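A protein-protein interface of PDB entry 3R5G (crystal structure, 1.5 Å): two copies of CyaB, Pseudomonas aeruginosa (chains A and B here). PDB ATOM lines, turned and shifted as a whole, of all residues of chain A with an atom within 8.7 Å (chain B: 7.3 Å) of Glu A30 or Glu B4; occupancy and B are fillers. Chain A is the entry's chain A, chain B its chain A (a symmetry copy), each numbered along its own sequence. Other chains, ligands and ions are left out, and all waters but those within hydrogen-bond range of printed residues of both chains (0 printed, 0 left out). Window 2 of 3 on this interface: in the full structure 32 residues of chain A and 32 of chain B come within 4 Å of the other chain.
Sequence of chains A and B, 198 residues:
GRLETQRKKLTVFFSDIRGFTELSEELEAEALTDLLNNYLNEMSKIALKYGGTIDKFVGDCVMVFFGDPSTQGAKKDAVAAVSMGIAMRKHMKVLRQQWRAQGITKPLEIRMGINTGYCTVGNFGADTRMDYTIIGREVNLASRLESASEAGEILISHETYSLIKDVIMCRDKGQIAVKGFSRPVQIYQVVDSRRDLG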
ATOM      1  N   LEU A  27      -1.743  27.745 -17.513  1.00  0.00           N
ATOM      2  CA  LEU A  27      -2.911  27.545 -18.383  1.00  0.00           C
ATOM      3  C   LEU A  27      -4.191  28.021 -17.732  1.00  0.00           C
ATOM      4  O   LEU A  27      -4.398  27.791 -16.553  1.00  0.00           O
ATOM      5  CB  LEU A  27      -3.084  26.051 -18.689  1.00  0.00           C
ATOM      6  CG  LEU A  27      -2.516  25.523 -19.986  1.00  0.00           C
ATOM      7  CD1 LEU A  27      -2.962  24.097 -20.194  1.00  0.00           C
ATOM      8  CD2 LEU A  27      -2.980  26.425 -21.148  1.00  0.00           C
ATOM      9  N   GLU A  28      -5.075  28.662 -18.496  1.00  0.00           N
ATOM     10  CA  GLU A  28      -6.466  28.878 -18.057  1.00  0.00           C
ATOM     11  C   GLU A  28      -7.016  27.556 -17.513  1.00  0.00           C
ATOM     12  O   GLU A  28      -6.675  26.486 -18.038  1.00  0.00           O
ATOM     13  CB  GLU A  28      -7.328  29.352 -19.254  1.00  0.00           C
ATOM     14  CG  GLU A  28      -8.352  30.484 -18.969  1.00  0.00           C
ATOM     15  CD  GLU A  28      -9.771  29.958 -18.624  1.00  0.00           C
ATOM     16  OE1 GLU A  28      -9.922  29.302 -17.547  1.00  0.00           O
ATOM     17  OE2 GLU A  28     -10.729  30.229 -19.424  1.00  0.00           O
ATOM     18  N   ALA A  29      -7.831  27.617 -16.461  1.00  0.00           N
ATOM     19  CA  ALA A  29      -8.385  26.411 -15.845  1.00  0.00           C
ATOM     20  C   ALA A  29      -9.162  25.542 -16.851  1.00  0.00           C
ATOM     21  O   ALA A  29      -9.142  24.310 -16.750  1.00  0.00           O
ATOM     22  CB  ALA A  29      -9.248  26.755 -14.625  1.00  0.00           C
ATOM     23  N   GLU A  30      -9.848  26.177 -17.805  1.00  0.00           N
ATOM     24  CA  GLU A  30     -10.661  25.398 -18.742  1.00  0.00           C
ATOM     25  C   GLU A  30      -9.775  24.623 -19.779  1.00  0.00           C
ATOM     26  O   GLU A  30     -10.031  23.444 -20.049  1.00  0.00           O
ATOM     27  CB  GLU A  30     -11.743  26.258 -19.413  1.00  0.00           C
ATOM     28  CG  GLU A  30     -12.721  25.442 -20.267  1.00  0.00           C
ATOM     29  CD  GLU A  30     -13.249  26.195 -21.514  1.00  0.00           C
ATOM     30  OE1 GLU A  30     -12.696  27.270 -21.881  1.00  0.00           O
ATOM     31  OE2 GLU A  30     -14.212  25.677 -22.138  1.00  0.00           O
ATOM     32  N   ALA A  31      -8.758  25.296 -20.329  1.00  0.00           N
ATOM     33  CA  ALA A  31      -7.784  24.667 -21.229  1.00  0.00           C
ATOM     34  C   ALA A  31      -7.014  23.558 -20.456  1.00  0.00           C
ATOM     35  O   ALA A  31      -6.815  22.470 -20.984  1.00  0.00           O
ATOM     36  CB  ALA A  31      -6.856  25.649 -21.765  1.00  0.00           C
ATOM     37  N   LEU A  32      -6.619  23.841 -19.211  1.00  0.00           N
ATOM     38  CA  LEU A  32      -5.972  22.791 -18.356  1.00  0.00           C
ATOM     39  C   LEU A  32      -6.856  21.559 -18.149  1.00  0.00           C
ATOM     40  O   LEU A  32      -6.369  20.415 -18.317  1.00  0.00           O
ATOM     41  CB  LEU A  32      -5.512  23.423 -17.034  1.00  0.00           C
ATOM     42  CG  LEU A  32      -4.864  22.508 -15.979  1.00  0.00           C
ATOM     43  CD1 LEU A  32      -3.556  21.924 -16.513  1.00  0.00           C
ATOM     44  CD2 LEU A  32      -4.591  23.283 -14.661  1.00  0.00           C
ATOM     45  N   THR A  33      -8.130  21.754 -17.776  1.00  0.00           N
ATOM     46  CA  THR A  33      -9.080  20.724 -17.648  1.00  0.00           C
ATOM     47  C   THR A  33      -9.205  19.917 -18.934  1.00  0.00           C
ATOM     48  O   THR A  33      -9.183  18.679 -18.894  1.00  0.00           O
ATOM     49  CB  THR A  33     -10.477  21.305 -17.225  1.00  0.00           C
ATOM     50  OG1 THR A  33     -10.311  21.903 -15.949  1.00  0.00           O
ATOM     51  CG2 THR A  33     -11.509  20.243 -17.130  1.00  0.00           C
ATOM     52  N   ASP A  34      -9.370  20.590 -20.082  1.00  0.00           N
ATOM     53  CA  ASP A  34      -9.511  19.834 -21.304  1.00  0.00           C
ATOM     54  C   ASP A  34      -8.212  19.032 -21.652  1.00  0.00           C
ATOM     55  O   ASP A  34      -8.350  17.893 -22.111  1.00  0.00           O
ATOM     56  CB  ASP A  34      -9.839  20.812 -22.462  1.00  0.00           C
ATOM     57  CG  ASP A  34     -11.235  21.339 -22.406  1.00  0.00           C
ATOM     58  OD1 ASP A  34     -12.141  20.654 -21.865  1.00  0.00           O
ATOM     59  OD2 ASP A  34     -11.439  22.439 -22.999  1.00  0.00           O
ATOM     60  N   LEU A  35      -7.054  19.620 -21.475  1.00  0.00           N
ATOM     61  CA  LEU A  35      -5.775  18.942 -21.755  1.00  0.00           C
ATOM     62  C   LEU A  35      -5.574  17.753 -20.804  1.00  0.00           C
ATOM     63  O   LEU A  35      -5.296  16.674 -21.291  1.00  0.00           O
ATOM     64  CB  LEU A  35      -4.654  19.912 -21.657  1.00  0.00           C
ATOM     65  CG  LEU A  35      -3.281  19.217 -21.910  1.00  0.00           C
ATOM     66  CD1 LEU A  35      -2.535  20.196 -22.602  1.00  0.00           C
ATOM     67  CD2 LEU A  35      -2.523  18.788 -20.632  1.00  0.00           C
ATOM     68  N   LEU A  36      -5.750  17.968 -19.493  1.00  0.00           N
ATOM     69  CA  LEU A  36      -5.631  16.785 -18.585  1.00  0.00           C
ATOM     70  C   LEU A  36      -6.681  15.711 -18.925  1.00  0.00           C
ATOM     71  O   LEU A  36      -6.400  14.467 -18.884  1.00  0.00           O
ATOM     72  CB  LEU A  36      -5.762  17.206 -17.114  1.00  0.00           C
ATOM     73  CG  LEU A  36      -5.755  16.122 -16.029  1.00  0.00           C
ATOM     74  CD1 LEU A  36      -4.407  15.313 -16.161  1.00  0.00           C
ATOM     75  CD2 LEU A  36      -5.809  16.796 -14.632  1.00  0.00           C
ATOM     76  N   ASN A  37      -7.998  16.051 -19.103  1.00  0.00           N
ATOM     77  CA  ASN A  37      -8.980  15.053 -19.317  1.00  0.00           C
ATOM     78  C   ASN A  37      -8.779  14.284 -20.654  1.00  0.00           C
ATOM     79  O   ASN A  37      -9.070  13.089 -20.692  1.00  0.00           O
ATOM     80  CB  ASN A  37     -10.425  15.655 -19.188  1.00  0.00           C
ATOM     81  CG  ASN A  37     -10.741  16.100 -17.769  1.00  0.00           C
ATOM     82  OD1 ASN A  37      -9.985  15.859 -16.880  1.00  0.00           O
ATOM     83  ND2 ASN A  37     -11.808  16.880 -17.584  1.00  0.00           N
ATOM     84  N   GLN A 102      -2.327  23.730 -30.472  1.00  0.00           N
ATOM     85  CA  GLN A 102      -3.140  24.681 -29.715  1.00  0.00           C
ATOM     86  C   GLN A 102      -2.248  25.732 -29.124  1.00  0.00           C
ATOM     87  O   GLN A 102      -2.696  26.528 -28.319  1.00  0.00           O
ATOM     88  CB  GLN A 102      -3.867  24.047 -28.532  1.00  0.00           C
ATOM     89  CG  GLN A 102      -4.550  22.727 -28.713  1.00  0.00           C
ATOM     90  CD  GLN A 102      -4.810  22.068 -27.336  1.00  0.00           C
ATOM     91  OE1 GLN A 102      -4.548  20.880 -27.153  1.00  0.00           O
ATOM     92  NE2 GLN A 102      -5.311  22.858 -26.355  1.00  0.00           N
ATOM     93  N   GLU B   4     -17.853  23.330 -13.084  1.00  0.00           N
ATOM     94  CA  GLU B   4     -16.779  24.057 -13.835  1.00  0.00           C
ATOM     95  C   GLU B   4     -15.503  24.393 -12.990  1.00  0.00           C
ATOM     96  O   GLU B   4     -15.587  25.002 -11.930  1.00  0.00           O
ATOM     97  CB  GLU B   4     -17.341  25.331 -14.485  1.00  0.00           C
ATOM     98  CG  GLU B   4     -16.280  26.323 -15.019  1.00  0.00           C
ATOM     99  CD  GLU B   4     -15.766  26.033 -16.447  1.00  0.00           C
ATOM    100  OE1 GLU B   4     -16.448  25.323 -17.235  1.00  0.00           O
ATOM    101  OE2 GLU B   4     -14.667  26.560 -16.799  1.00  0.00           O
ATOM    102  N   THR B   5     -14.332  24.061 -13.523  1.00  0.00           N
ATOM    103  CA  THR B   5     -12.988  24.274 -12.868  1.00  0.00           C
ATOM    104  C   THR B   5     -12.574  25.717 -12.444  1.00  0.00           C
ATOM    105  O   THR B   5     -12.589  26.648 -13.253  1.00  0.00           O
ATOM    106  CB  THR B   5     -11.883  23.689 -13.830  1.00  0.00           C
ATOM    107  OG1 THR B   5     -12.287  22.378 -14.238  1.00  0.00           O
ATOM    108  CG2 THR B   5     -10.516  23.645 -13.117  1.00  0.00           C
ATOM    109  N   GLN B   6     -12.087  25.899 -11.187  1.00  0.00           N
ATOM    110  CA  GLN B   6     -11.679  27.227 -10.685  1.00  0.00           C
ATOM    111  C   GLN B   6     -10.326  27.236  -9.983  1.00  0.00           C
ATOM    112  O   GLN B   6      -9.859  26.167  -9.653  1.00  0.00           O
ATOM    113  CB  GLN B   6     -12.676  27.783  -9.681  1.00  0.00           C
ATOM    114  CG  GLN B   6     -13.602  26.812  -9.080  1.00  0.00           C
ATOM    115  CD  GLN B   6     -15.049  27.362  -9.082  1.00  0.00           C
ATOM    116  OE1 GLN B   6     -15.738  27.314 -10.101  1.00  0.00           O
ATOM    117  NE2 GLN B   6     -15.500  27.880  -7.943  1.00  0.00           N
ATOM    118  N   ARG B   7      -9.736  28.404  -9.822  1.00  0.00           N
ATOM    119  CA  ARG B   7      -8.463  28.587  -9.072  1.00  0.00           C
ATOM    120  C   ARG B   7      -8.866  29.197  -7.764  1.00  0.00           C
ATOM    121  O   ARG B   7      -9.510  30.229  -7.768  1.00  0.00           O
ATOM    122  CB  ARG B   7      -7.546  29.564  -9.788  1.00  0.00           C
ATOM    123  CG  ARG B   7      -6.121  29.505  -9.297  1.00  0.00           C
ATOM    124  CD  ARG B   7      -5.138  29.306 -10.455  1.00  0.00           C
ATOM    125  NE  ARG B   7      -3.768  29.492  -9.986  1.00  0.00           N
ATOM    126  CZ  ARG B   7      -3.365  30.577  -9.327  1.00  0.00           C
ATOM    127  NH1 ARG B   7      -4.235  31.552  -9.085  1.00  0.00           N
ATOM    128  NH2 ARG B   7      -2.091  30.690  -8.906  1.00  0.00           N
ATOM    129  N   THR B 120      -5.971  24.602  -8.395  1.00  0.00           N
ATOM    130  CA  THR B 120      -7.049  24.457  -9.418  1.00  0.00           C
ATOM    131  C   THR B 120      -7.939  23.319  -8.991  1.00  0.00           C
ATOM    132  O   THR B 120      -7.493  22.156  -8.738  1.00  0.00           O
ATOM    133  CB  THR B 120      -6.440  24.160 -10.789  1.00  0.00           C
ATOM    134  OG1 THR B 120      -5.502  25.185 -11.123  1.00  0.00           O
ATOM    135  CG2 THR B 120      -7.534  23.934 -11.837  1.00  0.00           C
ATOM    136  N   VAL B 121      -9.255  23.586  -8.940  1.00  0.00           N
ATOM    137  CA  VAL B 121     -10.219  22.557  -8.490  1.00  0.00           C
ATOM    138  C   VAL B 121     -11.269  22.285  -9.557  1.00  0.00           C
ATOM    139  O   VAL B 121     -11.745  23.223 -10.172  1.00  0.00           O
ATOM    140  CB  VAL B 121     -11.131  22.962  -7.284  1.00  0.00           C
ATOM    141  CG1 VAL B 121     -11.657  21.662  -6.495  1.00  0.00           C
ATOM    142  CG2 VAL B 121     -10.441  23.995  -6.463  1.00  0.00           C
ATOM    143  N   GLY B 122     -11.590  21.053  -9.772  1.00  0.00           N
ATOM    144  CA  GLY B 122     -12.472  20.773 -10.935  1.00  0.00           C
ATOM    145  C   GLY B 122     -12.756  19.330 -11.046  1.00  0.00           C
ATOM    146  O   GLY B 122     -12.358  18.514 -10.218  1.00  0.00           O
ATOM    147  N   ASN B 123     -13.467  18.948 -12.135  1.00  0.00           N
ATOM    148  CA  ASN B 123     -13.701  17.570 -12.381  1.00  0.00           C
ATOM    149  C   ASN B 123     -12.692  17.082 -13.406  1.00  0.00           C
ATOM    150  O   ASN B 123     -12.631  17.605 -14.531  1.00  0.00           O
ATOM    151  CB  ASN B 123     -15.143  17.334 -12.931  1.00  0.00           C
ATOM    152  CG  ASN B 123     -16.160  17.737 -11.942  1.00  0.00           C
ATOM    153  OD1 ASN B 123     -16.277  17.115 -10.871  1.00  0.00           O
ATOM    154  ND2 ASN B 123     -16.909  18.789 -12.262  1.00  0.00           N
ATOM    155  N   TYR B 132     -14.030  14.843  -8.735  1.00  0.00           N
ATOM    156  CA  TYR B 132     -13.880  16.240  -8.333  1.00  0.00           C
ATOM    157  C   TYR B 132     -12.676  16.319  -7.412  1.00  0.00           C
ATOM    158  O   TYR B 132     -12.637  15.596  -6.403  1.00  0.00           O
ATOM    159  CB  TYR B 132     -15.123  16.568  -7.461  1.00  0.00           C
ATOM    160  CG  TYR B 132     -15.191  17.960  -7.154  1.00  0.00           C
ATOM    161  CD1 TYR B 132     -15.678  18.897  -8.091  1.00  0.00           C
ATOM    162  CD2 TYR B 132     -14.697  18.433  -5.940  1.00  0.00           C
ATOM    163  CE1 TYR B 132     -15.737  20.228  -7.805  1.00  0.00           C
ATOM    164  CE2 TYR B 132     -14.772  19.742  -5.623  1.00  0.00           C
ATOM    165  CZ  TYR B 132     -15.262  20.676  -6.535  1.00  0.00           C
ATOM    166  OH  TYR B 132     -15.372  22.006  -6.318  1.00  0.00           O
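No position is printed for both chains.
Among the printed residues, merely in contact across the chains: Ala A29 with Thr B5 (3.6 Å), Thr A33 with Asn B123 (3.9 Å) and Glu A30 with Glu B4 (3.9 Å).
The side-chain hydroxyl (OG1) of Thr B5 is in hydrogen-bond range of the side-chain hydroxyl (OG1) of Thr A33 (2.7 Å).
ND2 of Asn A37 sits at hydrogen-bond distance from O of Asn B123 (3.2 Å).
Of chain B, only Glu B4 (3.9 Å) comes within 4 Å of Glu A30.
Printed residues of chain A within 4 Å of Glu B4: Glu A30 (3.9 Å).
Printed residues of chain A within 4 Å of Thr B5: Ala A29 (3.6 Å) and Thr A33 (2.7 Å).
Printed residues of chain B within 4 Å of Ala A29: Thr B5 (3.6 Å).
Of the printed residues of chain A, Asn B123 touches Thr A33 (3.9 Å) and Asn A37 (3.2 Å).
Printed residues of chain B within 4 Å of Thr A33: Thr B5 (2.7 Å) and Asn B123 (3.9 Å).
Of the printed residues of chain B, Asn A37 touches Asn B123.
Gly B122 touches none of the printed residues of chain A.
The nearest residue of chain A that does not touch Glu B4 is Glu A28 (5.5 Å).
Of the 9 printed residues of chain B, 3 touch a printed residue of chain A.
Printed residues of chain B that touch a printed residue of chain A: Glu B4, Thr B5 and Asn B123.
Hydrophobic or aromatic side chains of chain A that line the printed part of chain B: Ala A29.
Among the printed residues, 5 pairs touch across the chains.
Among the printed residues, no Asp or Glu carboxylate lies within 4 Å of a Lys or Arg side-chain nitrogen of the other chain.
The side-chain amide nitrogen (ND2) of Asn A37 lies close to the backbone carbonyl oxygen (O) of Thr A33, at 3.4 Å.
The side-chain amide oxygen (OE1) of Gln B6 lies close to the backbone carbonyl oxygen (O) of Glu B4.
The backbone NH of Glu A30 lies within hydrogen-bond range of the side-chain carboxylate of Glu A28 (3.1 Å).
The backbone carbonyl oxygen of Ala A29 is in hydrogen-bond range of the side-chain hydroxyl of Thr A33 (2.8 Å).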
